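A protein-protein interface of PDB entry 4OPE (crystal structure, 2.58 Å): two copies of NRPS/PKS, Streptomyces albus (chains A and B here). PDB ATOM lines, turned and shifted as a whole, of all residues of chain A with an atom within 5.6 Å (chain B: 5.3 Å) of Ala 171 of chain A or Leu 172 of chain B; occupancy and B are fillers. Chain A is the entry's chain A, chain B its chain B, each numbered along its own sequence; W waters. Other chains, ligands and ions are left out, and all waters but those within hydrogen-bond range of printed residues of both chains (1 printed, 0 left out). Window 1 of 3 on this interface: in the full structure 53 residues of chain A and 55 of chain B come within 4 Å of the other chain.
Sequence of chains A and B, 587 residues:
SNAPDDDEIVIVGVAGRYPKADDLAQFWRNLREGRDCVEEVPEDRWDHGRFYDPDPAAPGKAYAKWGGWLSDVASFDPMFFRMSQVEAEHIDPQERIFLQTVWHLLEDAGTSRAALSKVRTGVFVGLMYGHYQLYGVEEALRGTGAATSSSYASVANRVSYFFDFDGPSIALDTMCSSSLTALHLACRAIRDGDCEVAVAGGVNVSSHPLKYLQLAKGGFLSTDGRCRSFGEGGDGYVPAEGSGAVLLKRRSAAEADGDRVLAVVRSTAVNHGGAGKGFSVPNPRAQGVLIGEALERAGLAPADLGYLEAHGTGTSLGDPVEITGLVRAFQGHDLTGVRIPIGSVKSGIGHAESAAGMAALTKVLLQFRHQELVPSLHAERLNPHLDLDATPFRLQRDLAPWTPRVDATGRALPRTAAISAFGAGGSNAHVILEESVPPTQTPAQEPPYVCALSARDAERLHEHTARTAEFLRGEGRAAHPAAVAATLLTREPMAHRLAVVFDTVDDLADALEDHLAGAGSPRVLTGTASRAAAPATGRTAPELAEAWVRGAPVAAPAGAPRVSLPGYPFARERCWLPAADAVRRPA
N of Ala 153 of chain A lies within hydrogen-bond range of OD2 of Asp 173 of chain B (2.9 Å). O of Ala 171 of chain A lies within hydrogen-bond range of N of Asp 173 of chain B. N of Asp 173 of chain A sits at hydrogen-bond distance from O of Ala 171 of chain B (2.9 Å).
O of Val 123 of chain A lies within hydrogen-bond range of N of Ile 170 of chain A (2.9 Å). The backbone NH (N) of Val 125 of chain A sits at hydrogen-bond distance from the backbone carbonyl oxygen (O) of Ile 170 of chain A, 3.2 Å away. The backbone NH (N) of Leu 127 of chain A is in hydrogen-bond range of the backbone carbonyl oxygen (O) of Leu 172 of chain A, 2.9 Å away. O of Ala 156 of chain A sits close to OG of Ser 169 of chain A, at 3.3 Å. O of Leu 172 of chain B lies within hydrogen-bond range of N of Leu 127 of chain B. OG1 of Thr 181 of chain B sits at hydrogen-bond distance from OG1 of Thr 174 of chain B (2.9 Å).
Among the printed residues, merely in contact across the chains: Tyr 152 of chain A with Asp 173 of chain B (3.5 Å), Ala 153 of chain A with Thr 174 of chain B (3.96 Å), Ser 169 of chain A with Thr 174 of chain B (3.5 Å), Ile 170 of chain A with Thr 174 of chain B (3.96 Å), Ile 170 of chain A with Thr 181 of chain B (3.96 Å), Ala 171 of chain A with Leu 172 of chain B (3.4 Å) and Leu 172 of chain A with Ala 171 of chain B (3.3 Å).
Printed residues of chain B within 4 Å of Tyr 152 of chain A: Asp 173 (3.5 Å). Of the printed residues of chain B, Ala 153 of chain A touches Asp 173 and Thr 174. Printed residues of chain B within 4 Å of Ile 170 of chain A: Thr 174 (3.96 Å) and Thr 181 (3.96 Å). Of chain B, only Leu 172 (3.4 Å) and Asp 173 (3.0 Å) come within 4 Å of Ala 171 of chain A. Printed residues of chain B within 4 Å of Leu 172 of chain A: Ala 171 (3.3 Å). Gly 126 of chain B touches none of the printed residues of chain A. Of chain A, only Ala 171 (3.4 Å) comes within 4 Å of Leu 172 of chain B. Printed residues of chain A within 4 Å of Thr 174 of chain B: Ala 153 (3.96 Å), Ser 169 (3.5 Å) and Ile 170 (3.96 Å). The nearest residue of chain B that does not touch Ala 171 of chain A is Ala 171 of chain B (4.4 Å).
Printed residues of chain B that touch a printed residue of chain A: Ala 171, Leu 172, Asp 173, Thr 174 and Thr 181. Hydrophobic or aromatic side chains of chain B that line the printed part of chain A: Ala 171 and Leu 172. Printed residues of chain A that touch a printed residue of chain B: Tyr 152, Ala 153, Ser 169, Ile 170, Ala 171, Leu 172 and Asp 173. Hydrophobic or aromatic side chains of chain A that line the printed part of chain B: Tyr 152, Ala 153, Ile 170, Ala 171 and Leu 172.
Ala 171 of chain A touches Leu 172 of chain B, and with the chains exchanged Leu 172 of chain A touches Ala 171 of chain B. Ala 171 of chain A touches Asp 173 of chain B, and with the chains exchanged Asp 173 of chain A touches Ala 171 of chain B. Positions printed for both chains: 125, 126, 127, 170, 171, 172 and 173.
Water W1 lies within hydrogen-bond range of the side-chain carboxylate of Asp 173 of chain B and the backbone NH of Tyr 152 of chain A.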
ATOM      1  N   VAL A 123       6.151 -10.256   8.180  1.00  0.00           N
ATOM      2  CA  VAL A 123       5.447 -11.532   8.403  1.00  0.00           C
ATOM      3  C   VAL A 123       4.347 -11.324   9.414  1.00  0.00           C
ATOM      4  O   VAL A 123       4.588 -10.743  10.486  1.00  0.00           O
ATOM      5  CB  VAL A 123       6.378 -12.555   8.987  1.00  0.00           C
ATOM      6  CG1 VAL A 123       5.626 -13.832   9.311  1.00  0.00           C
ATOM      7  CG2 VAL A 123       7.509 -12.813   8.018  1.00  0.00           C
ATOM      8  N   VAL A 125       0.927 -13.678  10.746  1.00  0.00           N
ATOM      9  CA  VAL A 125       0.364 -15.029  10.748  1.00  0.00           C
ATOM     10  C   VAL A 125      -0.657 -15.153  11.809  1.00  0.00           C
ATOM     11  O   VAL A 125      -0.420 -14.754  12.929  1.00  0.00           O
ATOM     12  CB  VAL A 125       1.460 -16.097  10.963  1.00  0.00           C
ATOM     13  CG1 VAL A 125       2.175 -15.936  12.296  1.00  0.00           C
ATOM     14  CG2 VAL A 125       0.914 -17.515  10.766  1.00  0.00           C
ATOM     15  N   GLY A 126      -1.815 -15.706  11.462  1.00  0.00           N
ATOM     16  CA  GLY A 126      -2.894 -15.862  12.444  1.00  0.00           C
ATOM     17  C   GLY A 126      -2.949 -17.260  12.986  1.00  0.00           C
ATOM     18  O   GLY A 126      -2.838 -18.254  12.228  1.00  0.00           O
ATOM     19  N   LEU A 127      -3.113 -17.345  14.305  1.00  0.00           N
ATOM     20  CA  LEU A 127      -3.345 -18.627  15.007  1.00  0.00           C
ATOM     21  C   LEU A 127      -4.340 -18.411  16.127  1.00  0.00           C
ATOM     22  O   LEU A 127      -4.476 -17.285  16.633  1.00  0.00           O
ATOM     23  CB  LEU A 127      -2.060 -19.106  15.615  1.00  0.00           C
ATOM     24  CG  LEU A 127      -0.840 -19.171  14.693  1.00  0.00           C
ATOM     25  CD1 LEU A 127       0.137 -18.066  15.014  1.00  0.00           C
ATOM     26  CD2 LEU A 127      -0.136 -20.491  14.904  1.00  0.00           C
ATOM     27  N   TYR A 152       3.086 -18.465  19.887  1.00  0.00           N
ATOM     28  CA  TYR A 152       2.532 -17.930  18.655  1.00  0.00           C
ATOM     29  C   TYR A 152       3.571 -17.039  17.988  1.00  0.00           C
ATOM     30  O   TYR A 152       3.831 -17.194  16.815  1.00  0.00           O
ATOM     31  CB  TYR A 152       1.233 -17.141  18.852  1.00  0.00           C
ATOM     32  CG  TYR A 152      -0.012 -17.933  19.218  1.00  0.00           C
ATOM     33  CD1 TYR A 152      -0.035 -19.312  19.232  1.00  0.00           C
ATOM     34  CD2 TYR A 152      -1.200 -17.270  19.531  1.00  0.00           C
ATOM     35  CE1 TYR A 152      -1.201 -19.995  19.531  1.00  0.00           C
ATOM     36  CE2 TYR A 152      -2.369 -17.945  19.875  1.00  0.00           C
ATOM     37  CZ  TYR A 152      -2.373 -19.301  19.876  1.00  0.00           C
ATOM     38  OH  TYR A 152      -3.540 -19.983  20.222  1.00  0.00           O
ATOM     39  N   ALA A 153       4.189 -16.128  18.725  1.00  0.00           N
ATOM     40  CA  ALA A 153       5.266 -15.318  18.161  1.00  0.00           C
ATOM     41  C   ALA A 153       6.331 -16.165  17.525  1.00  0.00           C
ATOM     42  O   ALA A 153       6.898 -15.759  16.514  1.00  0.00           O
ATOM     43  CB  ALA A 153       5.903 -14.492  19.222  1.00  0.00           C
ATOM     44  N   VAL A 155       6.029 -18.851  15.730  1.00  0.00           N
ATOM     45  CA  VAL A 155       5.645 -19.110  14.389  1.00  0.00           C
ATOM     46  C   VAL A 155       6.052 -17.959  13.421  1.00  0.00           C
ATOM     47  O   VAL A 155       6.597 -18.216  12.309  1.00  0.00           O
ATOM     48  CB  VAL A 155       4.156 -19.384  14.286  1.00  0.00           C
ATOM     49  CG1 VAL A 155       3.832 -19.758  12.857  1.00  0.00           C
ATOM     50  CG2 VAL A 155       3.751 -20.501  15.243  1.00  0.00           C
ATOM     51  N   ALA A 156       5.815 -16.705  13.800  1.00  0.00           N
ATOM     52  CA  ALA A 156       6.219 -15.639  12.907  1.00  0.00           C
ATOM     53  C   ALA A 156       7.743 -15.423  12.945  1.00  0.00           C
ATOM     54  O   ALA A 156       8.391 -15.315  11.900  1.00  0.00           O
ATOM     55  CB  ALA A 156       5.492 -14.375  13.236  1.00  0.00           C
ATOM     56  N   SER A 169       7.284  -8.623  12.462  1.00  0.00           N
ATOM     57  CA  SER A 169       7.091 -10.065  12.620  1.00  0.00           C
ATOM     58  C   SER A 169       6.077 -10.283  13.739  1.00  0.00           C
ATOM     59  O   SER A 169       6.418 -10.211  14.868  1.00  0.00           O
ATOM     60  CB  SER A 169       8.442 -10.801  12.936  1.00  0.00           C
ATOM     61  OG  SER A 169       8.293 -12.234  13.105  1.00  0.00           O
ATOM     62  N   ILE A 170       4.834 -10.589  13.397  1.00  0.00           N
ATOM     63  CA  ILE A 170       3.738 -10.564  14.339  1.00  0.00           C
ATOM     64  C   ILE A 170       2.853 -11.764  14.213  1.00  0.00           C
ATOM     65  O   ILE A 170       2.429 -12.085  13.114  1.00  0.00           O
ATOM     66  CB  ILE A 170       2.853  -9.353  14.018  1.00  0.00           C
ATOM     67  CG1 ILE A 170       3.711  -8.080  14.022  1.00  0.00           C
ATOM     68  CG2 ILE A 170       1.701  -9.276  15.026  1.00  0.00           C
ATOM     69  CD1 ILE A 170       2.938  -6.807  13.726  1.00  0.00           C
ATOM     70  N   ALA A 171       2.531 -12.412  15.310  1.00  0.00           N
ATOM     71  CA  ALA A 171       1.515 -13.438  15.280  1.00  0.00           C
ATOM     72  C   ALA A 171       0.281 -12.874  15.929  1.00  0.00           C
ATOM     73  O   ALA A 171       0.359 -12.011  16.816  1.00  0.00           O
ATOM     74  CB  ALA A 171       1.960 -14.687  16.003  1.00  0.00           C
ATOM     75  N   LEU A 172      -0.878 -13.332  15.513  1.00  0.00           N
ATOM     76  CA  LEU A 172      -2.094 -12.709  16.045  1.00  0.00           C
ATOM     77  C   LEU A 172      -3.265 -13.685  16.116  1.00  0.00           C
ATOM     78  O   LEU A 172      -3.347 -14.601  15.321  1.00  0.00           O
ATOM     79  CB  LEU A 172      -2.424 -11.427  15.283  1.00  0.00           C
ATOM     80  CG  LEU A 172      -2.604 -11.671  13.795  1.00  0.00           C
ATOM     81  CD1 LEU A 172      -4.079 -11.637  13.447  1.00  0.00           C
ATOM     82  CD2 LEU A 172      -1.861 -10.623  12.989  1.00  0.00           C
ATOM     83  N   ASP A 173      -4.096 -13.527  17.137  1.00  0.00           N
ATOM     84  CA  ASP A 173      -5.290 -14.327  17.326  1.00  0.00           C
ATOM     85  C   ASP A 173      -6.503 -13.397  17.291  1.00  0.00           C
ATOM     86  O   ASP A 173      -6.623 -12.508  18.117  1.00  0.00           O
ATOM     87  CB  ASP A 173      -5.186 -15.052  18.669  1.00  0.00           C
ATOM     88  CG  ASP A 173      -6.334 -16.023  18.929  1.00  0.00           C
ATOM     89  OD1 ASP A 173      -7.155 -16.237  18.001  1.00  0.00           O
ATOM     90  OD2 ASP A 173      -6.401 -16.560  20.083  1.00  0.00           O
ATOM     91  N   PHE B 124      -6.427  -3.478  21.243  1.00  0.00           N
ATOM     92  CA  PHE B 124      -5.196  -4.156  20.821  1.00  0.00           C
ATOM     93  C   PHE B 124      -4.456  -4.560  22.067  1.00  0.00           C
ATOM     94  O   PHE B 124      -4.070  -3.678  22.844  1.00  0.00           O
ATOM     95  CB  PHE B 124      -4.328  -3.185  20.049  1.00  0.00           C
ATOM     96  CG  PHE B 124      -4.997  -2.632  18.879  1.00  0.00           C
ATOM     97  CD1 PHE B 124      -5.816  -1.551  18.995  1.00  0.00           C
ATOM     98  CD2 PHE B 124      -4.842  -3.225  17.659  1.00  0.00           C
ATOM     99  CE1 PHE B 124      -6.489  -1.061  17.898  1.00  0.00           C
ATOM    100  CE2 PHE B 124      -5.484  -2.744  16.556  1.00  0.00           C
ATOM    101  CZ  PHE B 124      -6.319  -1.667  16.677  1.00  0.00           C
ATOM    102  N   VAL B 125      -4.238  -5.855  22.280  1.00  0.00           N
ATOM    103  CA  VAL B 125      -3.586  -6.299  23.513  1.00  0.00           C
ATOM    104  C   VAL B 125      -2.495  -7.364  23.281  1.00  0.00           C
ATOM    105  O   VAL B 125      -2.656  -8.301  22.475  1.00  0.00           O
ATOM    106  CB  VAL B 125      -4.638  -6.791  24.498  1.00  0.00           C
ATOM    107  CG1 VAL B 125      -5.395  -7.998  23.961  1.00  0.00           C
ATOM    108  CG2 VAL B 125      -4.022  -7.120  25.819  1.00  0.00           C
ATOM    109  N   GLY B 126      -1.362  -7.199  23.967  1.00  0.00           N
ATOM    110  CA  GLY B 126      -0.253  -8.099  23.792  1.00  0.00           C
ATOM    111  C   GLY B 126      -0.194  -9.159  24.861  1.00  0.00           C
ATOM    112  O   GLY B 126      -0.348  -8.846  26.025  1.00  0.00           O
ATOM    113  N   LEU B 127       0.040 -10.409  24.459  1.00  0.00           N
ATOM    114  CA  LEU B 127       0.211 -11.534  25.378  1.00  0.00           C
ATOM    115  C   LEU B 127       1.275 -12.439  24.824  1.00  0.00           C
ATOM    116  O   LEU B 127       1.422 -12.486  23.582  1.00  0.00           O
ATOM    117  CB  LEU B 127      -1.063 -12.360  25.421  1.00  0.00           C
ATOM    118  CG  LEU B 127      -2.299 -11.809  26.086  1.00  0.00           C
ATOM    119  CD1 LEU B 127      -3.222 -11.184  25.085  1.00  0.00           C
ATOM    120  CD2 LEU B 127      -3.014 -12.983  26.695  1.00  0.00           C
ATOM    121  N   ILE B 170      -8.103  -7.270  18.653  1.00  0.00           N
ATOM    122  CA  ILE B 170      -6.986  -8.048  18.219  1.00  0.00           C
ATOM    123  C   ILE B 170      -6.034  -8.351  19.324  1.00  0.00           C
ATOM    124  O   ILE B 170      -5.630  -7.470  20.048  1.00  0.00           O
ATOM    125  CB  ILE B 170      -6.188  -7.283  17.176  1.00  0.00           C
ATOM    126  CG1 ILE B 170      -7.094  -6.869  16.014  1.00  0.00           C
ATOM    127  CG2 ILE B 170      -5.050  -8.148  16.653  1.00  0.00           C
ATOM    128  CD1 ILE B 170      -6.348  -6.177  14.895  1.00  0.00           C
ATOM    129  N   ALA B 171      -5.666  -9.617  19.438  1.00  0.00           N
ATOM    130  CA  ALA B 171      -4.658 -10.033  20.372  1.00  0.00           C
ATOM    131  C   ALA B 171      -3.419 -10.378  19.572  1.00  0.00           C
ATOM    132  O   ALA B 171      -3.558 -11.076  18.570  1.00  0.00           O
ATOM    133  CB  ALA B 171      -5.124 -11.241  21.150  1.00  0.00           C
ATOM    134  N   LEU B 172      -2.242  -9.918  20.038  1.00  0.00           N
ATOM    135  CA  LEU B 172      -0.978 -10.216  19.369  1.00  0.00           C
ATOM    136  C   LEU B 172       0.147 -10.710  20.253  1.00  0.00           C
ATOM    137  O   LEU B 172       0.241 -10.358  21.408  1.00  0.00           O
ATOM    138  CB  LEU B 172      -0.491  -8.994  18.596  1.00  0.00           C
ATOM    139  CG  LEU B 172      -0.486  -7.678  19.343  1.00  0.00           C
ATOM    140  CD1 LEU B 172       0.718  -6.872  19.006  1.00  0.00           C
ATOM    141  CD2 LEU B 172      -1.718  -6.896  18.957  1.00  0.00           C
ATOM    142  N   ASP B 173       1.003 -11.569  19.712  1.00  0.00           N
ATOM    143  CA  ASP B 173       2.184 -12.010  20.464  1.00  0.00           C
ATOM    144  C   ASP B 173       3.418 -11.636  19.659  1.00  0.00           C
ATOM    145  O   ASP B 173       3.612 -12.114  18.567  1.00  0.00           O
ATOM    146  CB  ASP B 173       2.111 -13.528  20.700  1.00  0.00           C
ATOM    147  CG  ASP B 173       3.318 -14.088  21.403  1.00  0.00           C
ATOM    148  OD1 ASP B 173       4.128 -13.314  21.941  1.00  0.00           O
ATOM    149  OD2 ASP B 173       3.459 -15.322  21.418  1.00  0.00           O
ATOM    150  N   THR B 174       4.237 -10.752  20.183  1.00  0.00           N
ATOM    151  CA  THR B 174       5.602 -10.564  19.668  1.00  0.00           C
ATOM    152  C   THR B 174       6.611 -10.763  20.789  1.00  0.00           C
ATOM    153  O   THR B 174       7.721 -10.187  20.731  1.00  0.00           O
ATOM    154  CB  THR B 174       5.810  -9.181  19.017  1.00  0.00           C
ATOM    155  OG1 THR B 174       5.496  -8.094  19.916  1.00  0.00           O
ATOM    156  CG2 THR B 174       4.963  -9.062  17.791  1.00  0.00           C
ATOM    157  N   SER B 178       5.379  -7.242  22.919  1.00  0.00           N
ATOM    158  CA  SER B 178       3.966  -7.326  22.537  1.00  0.00           C
ATOM    159  C   SER B 178       3.156  -6.059  22.830  1.00  0.00           C
ATOM    160  O   SER B 178       2.450  -5.566  21.959  1.00  0.00           O
ATOM    161  CB  SER B 178       3.293  -8.544  23.173  1.00  0.00           C
ATOM    162  OG  SER B 178       3.895  -9.743  22.717  1.00  0.00           O
ATOM    163  N   THR B 181       4.149  -3.284  20.377  1.00  0.00           N
ATOM    164  CA  THR B 181       3.599  -3.656  19.073  1.00  0.00           C
ATOM    165  C   THR B 181       2.098  -3.300  19.068  1.00  0.00           C
ATOM    166  O   THR B 181       1.582  -2.757  18.075  1.00  0.00           O
ATOM    167  CB  THR B 181       3.818  -5.153  18.790  1.00  0.00           C
ATOM    168  OG1 THR B 181       5.229  -5.464  18.824  1.00  0.00           O
ATOM    169  CG2 THR B 181       3.272  -5.511  17.454  1.00  0.00           C
ATOM    170  N   ALA B 182       1.406  -3.580  20.178  1.00  0.00           N
ATOM    171  CA  ALA B 182      -0.009  -3.314  20.251  1.00  0.00           C
ATOM    172  C   ALA B 182      -0.243  -1.816  20.145  1.00  0.00           C
ATOM    173  O   ALA B 182      -1.129  -1.356  19.408  1.00  0.00           O
ATOM    174  CB  ALA B 182      -0.583  -3.857  21.535  1.00  0.00           C
ATOM    175  N   LEU B 185       0.175  -0.739  16.471  1.00  0.00           N
ATOM    176  CA  LEU B 185      -0.966  -1.070  15.635  1.00  0.00           C
ATOM    177  C   LEU B 185      -2.179  -0.243  15.972  1.00  0.00           C
ATOM    178  O   LEU B 185      -2.998   0.070  15.088  1.00  0.00           O
ATOM    179  CB  LEU B 185      -1.329  -2.554  15.779  1.00  0.00           C
ATOM    180  CG  LEU B 185      -0.298  -3.595  15.301  1.00  0.00           C
ATOM    181  CD1 LEU B 185      -0.843  -4.986  15.588  1.00  0.00           C
ATOM    182  CD2 LEU B 185       0.052  -3.492  13.818  1.00  0.00           C
HETATM  183  O   HOH W   1       2.395 -17.257  22.401  1.00  0.00           O
